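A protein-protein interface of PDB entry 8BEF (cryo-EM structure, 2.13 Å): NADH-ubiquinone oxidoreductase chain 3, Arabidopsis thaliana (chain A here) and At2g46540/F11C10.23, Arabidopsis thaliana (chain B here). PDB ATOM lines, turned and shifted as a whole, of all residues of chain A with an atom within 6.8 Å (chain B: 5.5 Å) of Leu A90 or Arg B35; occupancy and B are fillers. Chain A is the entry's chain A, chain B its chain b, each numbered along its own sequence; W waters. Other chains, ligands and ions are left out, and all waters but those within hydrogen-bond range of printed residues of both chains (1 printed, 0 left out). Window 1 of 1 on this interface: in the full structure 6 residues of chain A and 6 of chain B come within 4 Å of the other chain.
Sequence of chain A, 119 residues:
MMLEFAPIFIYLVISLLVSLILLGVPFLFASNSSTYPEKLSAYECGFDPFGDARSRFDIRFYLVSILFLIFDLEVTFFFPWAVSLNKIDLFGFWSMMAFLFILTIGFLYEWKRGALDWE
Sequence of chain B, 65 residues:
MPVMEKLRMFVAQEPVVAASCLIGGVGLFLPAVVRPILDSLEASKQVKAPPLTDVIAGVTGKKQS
The side-chain carboxylate of Asp A89 is in salt-bridge range of the guanidinium group of Arg B35, 3.5 Å away.
OD2 of Asp B39 lies within salt-bridge range of NE of Arg B35 (3.1 Å).
N of Arg B35 lies within hydrogen-bond range of O of Leu B30 (3.0 Å).
CG of Arg B35 touches CD1 of Leu A90, 3.9 Å away.
CE2 of Phe A93 touches CG of Pro B31 (3.4 Å).
CG of Pro B31 touches CZ2 of Trp A94, 3.8 Å away.
Ala B32 touches Trp A94.
Of chain B, only Arg B35 (3.9 Å) comes within 4 Å of Leu A90.
Arg B35 touches two residues of chain A.
Printed residues of chain B within 4 Å of Phe A93: Pro B31 (3.4 Å).
Of the printed residues of chain A, Ala B32 touches Trp A94 (3.7 Å).
Of the printed residues of chain A, Pro B31 touches Phe A93 and Trp A94.
The nearest residue of chain B that does not touch Leu A90 is Pro B31 (4.3 Å).
Of the 11 printed residues of chain B, 3 touch a printed residue of chain A.
Hydrophobic or aromatic side chains of chain B that line the printed part of chain A: Pro B31 and Ala B32.
Of the 10 printed residues of chain A, 4 touch a printed residue of chain B.
Along chain A the printed residues that touch a printed residue of chain B span positions 89 to 94.
Among the printed residues, 5 pairs touch across the chains.
Water W1 lies within hydrogen-bond range of the backbone carbonyl oxygen of Pro B31 (2.8 Å) and the indole nitrogen of Trp A94 (2.8 Å).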
ATOM      1  N   LEU A  85      13.894  -4.819 -20.178  1.00  0.00           N
ATOM      2  CA  LEU A  85      14.535  -3.510 -20.317  1.00  0.00           C
ATOM      3  C   LEU A  85      14.111  -2.527 -19.228  1.00  0.00           C
ATOM      4  O   LEU A  85      14.919  -1.689 -18.811  1.00  0.00           O
ATOM      5  CB  LEU A  85      14.234  -2.925 -21.695  1.00  0.00           C
ATOM      6  CG  LEU A  85      15.274  -3.214 -22.779  1.00  0.00           C
ATOM      7  CD1 LEU A  85      14.934  -2.466 -24.055  1.00  0.00           C
ATOM      8  CD2 LEU A  85      16.678  -2.856 -22.301  1.00  0.00           C
ATOM      9  N   LYS A  87      13.649  -2.996 -16.139  1.00  0.00           N
ATOM     10  CA  LYS A  87      14.308  -3.244 -14.864  1.00  0.00           C
ATOM     11  C   LYS A  87      15.829  -3.209 -14.937  1.00  0.00           C
ATOM     12  O   LYS A  87      16.469  -2.806 -13.963  1.00  0.00           O
ATOM     13  CB  LYS A  87      13.858  -4.593 -14.298  1.00  0.00           C
ATOM     14  CG  LYS A  87      12.436  -4.572 -13.771  1.00  0.00           C
ATOM     15  CD  LYS A  87      12.095  -5.847 -13.028  1.00  0.00           C
ATOM     16  CE  LYS A  87      12.368  -7.057 -13.893  1.00  0.00           C
ATOM     17  NZ  LYS A  87      11.209  -7.382 -14.767  1.00  0.00           N
ATOM     18  N   ILE A  88      16.429  -3.613 -16.059  1.00  0.00           N
ATOM     19  CA  ILE A  88      17.886  -3.659 -16.129  1.00  0.00           C
ATOM     20  C   ILE A  88      18.499  -2.307 -16.463  1.00  0.00           C
ATOM     21  O   ILE A  88      19.682  -2.091 -16.177  1.00  0.00           O
ATOM     22  CB  ILE A  88      18.360  -4.709 -17.149  1.00  0.00           C
ATOM     23  CG1 ILE A  88      17.884  -4.347 -18.560  1.00  0.00           C
ATOM     24  CG2 ILE A  88      17.901  -6.091 -16.734  1.00  0.00           C
ATOM     25  CD1 ILE A  88      18.036  -5.468 -19.562  1.00  0.00           C
ATOM     26  N   ASP A  89      17.739  -1.411 -17.082  1.00  0.00           N
ATOM     27  CA  ASP A  89      18.101   0.002 -17.296  1.00  0.00           C
ATOM     28  C   ASP A  89      19.377   0.076 -18.147  1.00  0.00           C
ATOM     29  O   ASP A  89      19.523  -0.683 -19.116  1.00  0.00           O
ATOM     30  CB  ASP A  89      18.189   0.708 -15.965  1.00  0.00           C
ATOM     31  CG  ASP A  89      18.055   2.210 -16.099  1.00  0.00           C
ATOM     32  OD1 ASP A  89      17.791   2.682 -17.225  1.00  0.00           O
ATOM     33  OD2 ASP A  89      18.213   2.918 -15.082  1.00  0.00           O
ATOM     34  N   LEU A  90      20.306   0.976 -17.816  1.00  0.00           N
ATOM     35  CA  LEU A  90      21.421   1.271 -18.710  1.00  0.00           C
ATOM     36  C   LEU A  90      22.439   0.139 -18.741  1.00  0.00           C
ATOM     37  O   LEU A  90      23.001  -0.164 -19.797  1.00  0.00           O
ATOM     38  CB  LEU A  90      22.088   2.581 -18.296  1.00  0.00           C
ATOM     39  CG  LEU A  90      21.401   3.846 -18.806  1.00  0.00           C
ATOM     40  CD1 LEU A  90      22.128   5.089 -18.324  1.00  0.00           C
ATOM     41  CD2 LEU A  90      21.303   3.825 -20.324  1.00  0.00           C
ATOM     42  N   PHE A  91      22.699  -0.486 -17.592  1.00  0.00           N
ATOM     43  CA  PHE A  91      23.695  -1.551 -17.532  1.00  0.00           C
ATOM     44  C   PHE A  91      23.310  -2.714 -18.439  1.00  0.00           C
ATOM     45  O   PHE A  91      24.143  -3.225 -19.196  1.00  0.00           O
ATOM     46  CB  PHE A  91      23.868  -2.026 -16.087  1.00  0.00           C
ATOM     47  CG  PHE A  91      25.118  -2.821 -15.853  1.00  0.00           C
ATOM     48  CD1 PHE A  91      25.214  -4.136 -16.283  1.00  0.00           C
ATOM     49  CD2 PHE A  91      26.198  -2.258 -15.192  1.00  0.00           C
ATOM     50  CE1 PHE A  91      26.358  -4.869 -16.067  1.00  0.00           C
ATOM     51  CE2 PHE A  91      27.346  -2.990 -14.969  1.00  0.00           C
ATOM     52  CZ  PHE A  91      27.428  -4.293 -15.410  1.00  0.00           C
ATOM     53  N   GLY A  92      22.050  -3.149 -18.370  1.00  0.00           N
ATOM     54  CA  GLY A  92      21.609  -4.244 -19.219  1.00  0.00           C
ATOM     55  C   GLY A  92      21.646  -3.883 -20.691  1.00  0.00           C
ATOM     56  O   GLY A  92      22.023  -4.704 -21.537  1.00  0.00           O
ATOM     57  N   PHE A  93      21.276  -2.641 -21.012  1.00  0.00           N
ATOM     58  CA  PHE A  93      21.323  -2.178 -22.393  1.00  0.00           C
ATOM     59  C   PHE A  93      22.734  -2.282 -22.958  1.00  0.00           C
ATOM     60  O   PHE A  93      22.939  -2.833 -24.043  1.00  0.00           O
ATOM     61  CB  PHE A  93      20.809  -0.738 -22.479  1.00  0.00           C
ATOM     62  CG  PHE A  93      20.950  -0.128 -23.843  1.00  0.00           C
ATOM     63  CD1 PHE A  93      19.974  -0.324 -24.808  1.00  0.00           C
ATOM     64  CD2 PHE A  93      22.062   0.634 -24.165  1.00  0.00           C
ATOM     65  CE1 PHE A  93      20.101   0.228 -26.065  1.00  0.00           C
ATOM     66  CE2 PHE A  93      22.197   1.189 -25.424  1.00  0.00           C
ATOM     67  CZ  PHE A  93      21.214   0.987 -26.375  1.00  0.00           C
ATOM     68  N   TRP A  94      23.726  -1.781 -22.218  1.00  0.00           N
ATOM     69  CA  TRP A  94      25.089  -1.774 -22.738  1.00  0.00           C
ATOM     70  C   TRP A  94      25.710  -3.167 -22.738  1.00  0.00           C
ATOM     71  O   TRP A  94      26.533  -3.469 -23.609  1.00  0.00           O
ATOM     72  CB  TRP A  94      25.948  -0.790 -21.947  1.00  0.00           C
ATOM     73  CG  TRP A  94      25.586   0.629 -22.258  1.00  0.00           C
ATOM     74  CD1 TRP A  94      25.021   1.534 -21.411  1.00  0.00           C
ATOM     75  CD2 TRP A  94      25.721   1.290 -23.522  1.00  0.00           C
ATOM     76  NE1 TRP A  94      24.814   2.726 -22.062  1.00  0.00           N
ATOM     77  CE2 TRP A  94      25.234   2.602 -23.361  1.00  0.00           C
ATOM     78  CE3 TRP A  94      26.218   0.904 -24.771  1.00  0.00           C
ATOM     79  CZ2 TRP A  94      25.228   3.530 -24.401  1.00  0.00           C
ATOM     80  CZ3 TRP A  94      26.210   1.826 -25.802  1.00  0.00           C
ATOM     81  CH2 TRP A  94      25.719   3.124 -25.610  1.00  0.00           C
ATOM     82  N   SER A  95      25.332  -4.028 -21.790  1.00  0.00           N
ATOM     83  CA  SER A  95      25.824  -5.402 -21.830  1.00  0.00           C
ATOM     84  C   SER A  95      25.306  -6.126 -23.070  1.00  0.00           C
ATOM     85  O   SER A  95      26.064  -6.829 -23.756  1.00  0.00           O
ATOM     86  CB  SER A  95      25.431  -6.149 -20.551  1.00  0.00           C
ATOM     87  OG  SER A  95      24.041  -6.403 -20.494  1.00  0.00           O
ATOM     88  N   LEU B  30      22.002   8.021 -28.655  1.00  0.00           N
ATOM     89  CA  LEU B  30      21.041   8.572 -27.701  1.00  0.00           C
ATOM     90  C   LEU B  30      21.330   8.156 -26.260  1.00  0.00           C
ATOM     91  O   LEU B  30      21.450   9.046 -25.402  1.00  0.00           O
ATOM     92  CB  LEU B  30      19.616   8.204 -28.126  1.00  0.00           C
ATOM     93  CG  LEU B  30      19.045   9.014 -29.290  1.00  0.00           C
ATOM     94  CD1 LEU B  30      17.893   8.258 -29.935  1.00  0.00           C
ATOM     95  CD2 LEU B  30      18.618  10.402 -28.842  1.00  0.00           C
ATOM     96  N   PRO B  31      21.485   6.869 -25.922  1.00  0.00           N
ATOM     97  CA  PRO B  31      21.807   6.532 -24.527  1.00  0.00           C
ATOM     98  C   PRO B  31      23.202   6.960 -24.108  1.00  0.00           C
ATOM     99  O   PRO B  31      23.418   7.247 -22.925  1.00  0.00           O
ATOM    100  CB  PRO B  31      21.659   5.005 -24.493  1.00  0.00           C
ATOM    101  CG  PRO B  31      21.924   4.592 -25.894  1.00  0.00           C
ATOM    102  CD  PRO B  31      21.278   5.652 -26.725  1.00  0.00           C
ATOM    103  N   ALA B  32      24.153   7.011 -25.041  1.00  0.00           N
ATOM    104  CA  ALA B  32      25.531   7.322 -24.676  1.00  0.00           C
ATOM    105  C   ALA B  32      25.706   8.801 -24.351  1.00  0.00           C
ATOM    106  O   ALA B  32      26.470   9.154 -23.448  1.00  0.00           O
ATOM    107  CB  ALA B  32      26.477   6.903 -25.799  1.00  0.00           C
ATOM    108  N   VAL B  33      25.008   9.676 -25.065  1.00  0.00           N
ATOM    109  CA  VAL B  33      25.204  11.116 -24.958  1.00  0.00           C
ATOM    110  C   VAL B  33      23.979  11.811 -24.373  1.00  0.00           C
ATOM    111  O   VAL B  33      24.087  12.557 -23.400  1.00  0.00           O
ATOM    112  CB  VAL B  33      25.583  11.722 -26.328  1.00  0.00           C
ATOM    113  CG1 VAL B  33      25.619  13.237 -26.244  1.00  0.00           C
ATOM    114  CG2 VAL B  33      26.918  11.172 -26.801  1.00  0.00           C
ATOM    115  N   VAL B  34      22.804  11.585 -24.963  1.00  0.00           N
ATOM    116  CA  VAL B  34      21.624  12.349 -24.573  1.00  0.00           C
ATOM    117  C   VAL B  34      21.152  11.950 -23.177  1.00  0.00           C
ATOM    118  O   VAL B  34      20.800  12.810 -22.360  1.00  0.00           O
ATOM    119  CB  VAL B  34      20.517  12.179 -25.630  1.00  0.00           C
ATOM    120  CG1 VAL B  34      19.206  12.778 -25.146  1.00  0.00           C
ATOM    121  CG2 VAL B  34      20.953  12.822 -26.945  1.00  0.00           C
ATOM    122  N   ARG B  35      21.142  10.651 -22.877  1.00  0.00           N
ATOM    123  CA  ARG B  35      20.664  10.192 -21.574  1.00  0.00           C
ATOM    124  C   ARG B  35      21.454  10.769 -20.403  1.00  0.00           C
ATOM    125  O   ARG B  35      20.823  11.237 -19.440  1.00  0.00           O
ATOM    126  CB  ARG B  35      20.649   8.660 -21.539  1.00  0.00           C
ATOM    127  CG  ARG B  35      20.484   8.067 -20.149  1.00  0.00           C
ATOM    128  CD  ARG B  35      19.088   8.292 -19.586  1.00  0.00           C
ATOM    129  NE  ARG B  35      18.957   7.677 -18.272  1.00  0.00           N
ATOM    130  CZ  ARG B  35      18.252   6.583 -18.022  1.00  0.00           C
ATOM    131  NH1 ARG B  35      17.543   5.985 -18.965  1.00  0.00           N
ATOM    132  NH2 ARG B  35      18.253   6.077 -16.793  1.00  0.00           N
ATOM    133  N   PRO B  36      22.795  10.753 -20.388  1.00  0.00           N
ATOM    134  CA  PRO B  36      23.500  11.422 -19.280  1.00  0.00           C
ATOM    135  C   PRO B  36      23.206  12.909 -19.195  1.00  0.00           C
ATOM    136  O   PRO B  36      23.170  13.460 -18.089  1.00  0.00           O
ATOM    137  CB  PRO B  36      24.982  11.152 -19.580  1.00  0.00           C
ATOM    138  CG  PRO B  36      25.036  10.709 -20.986  1.00  0.00           C
ATOM    139  CD  PRO B  36      23.733  10.044 -21.274  1.00  0.00           C
ATOM    140  N   ILE B  37      22.984  13.576 -20.329  1.00  0.00           N
ATOM    141  CA  ILE B  37      22.592  14.984 -20.304  1.00  0.00           C
ATOM    142  C   ILE B  37      21.246  15.149 -19.609  1.00  0.00           C
ATOM    143  O   ILE B  37      21.071  16.023 -18.753  1.00  0.00           O
ATOM    144  CB  ILE B  37      22.562  15.554 -21.734  1.00  0.00           C
ATOM    145  CG1 ILE B  37      23.977  15.636 -22.305  1.00  0.00           C
ATOM    146  CG2 ILE B  37      21.878  16.915 -21.759  1.00  0.00           C
ATOM    147  CD1 ILE B  37      24.020  15.994 -23.762  1.00  0.00           C
ATOM    148  N   LEU B  38      20.275  14.304 -19.964  1.00  0.00           N
ATOM    149  CA  LEU B  38      18.963  14.382 -19.332  1.00  0.00           C
ATOM    150  C   LEU B  38      19.042  14.055 -17.848  1.00  0.00           C
ATOM    151  O   LEU B  38      18.287  14.617 -17.049  1.00  0.00           O
ATOM    152  CB  LEU B  38      17.980  13.441 -20.033  1.00  0.00           C
ATOM    153  CG  LEU B  38      17.183  13.969 -21.232  1.00  0.00           C
ATOM    154  CD1 LEU B  38      18.026  14.852 -22.134  1.00  0.00           C
ATOM    155  CD2 LEU B  38      16.603  12.810 -22.021  1.00  0.00           C
ATOM    156  N   ASP B  39      19.945  13.152 -17.465  1.00  0.00           N
ATOM    157  CA  ASP B  39      20.125  12.835 -16.053  1.00  0.00           C
ATOM    158  C   ASP B  39      20.766  13.997 -15.304  1.00  0.00           C
ATOM    159  O   ASP B  39      20.435  14.252 -14.142  1.00  0.00           O
ATOM    160  CB  ASP B  39      20.965  11.567 -15.909  1.00  0.00           C
ATOM    161  CG  ASP B  39      20.271  10.342 -16.474  1.00  0.00           C
ATOM    162  OD1 ASP B  39      19.133  10.480 -16.966  1.00  0.00           O
ATOM    163  OD2 ASP B  39      20.864   9.244 -16.432  1.00  0.00           O
ATOM    164  N   SER B  40      21.687  14.711 -15.956  1.00  0.00           N
ATOM    165  CA  SER B  40      22.344  15.845 -15.313  1.00  0.00           C
ATOM    166  C   SER B  40      21.384  17.013 -15.126  1.00  0.00           C
ATOM    167  O   SER B  40      21.383  17.659 -14.073  1.00  0.00           O
ATOM    168  CB  SER B  40      23.559  16.276 -16.133  1.00  0.00           C
ATOM    169  OG  SER B  40      23.183  16.638 -17.450  1.00  0.00           O
HETATM  170  O   HOH W   1      24.580   5.413 -21.186  1.00  0.00           O
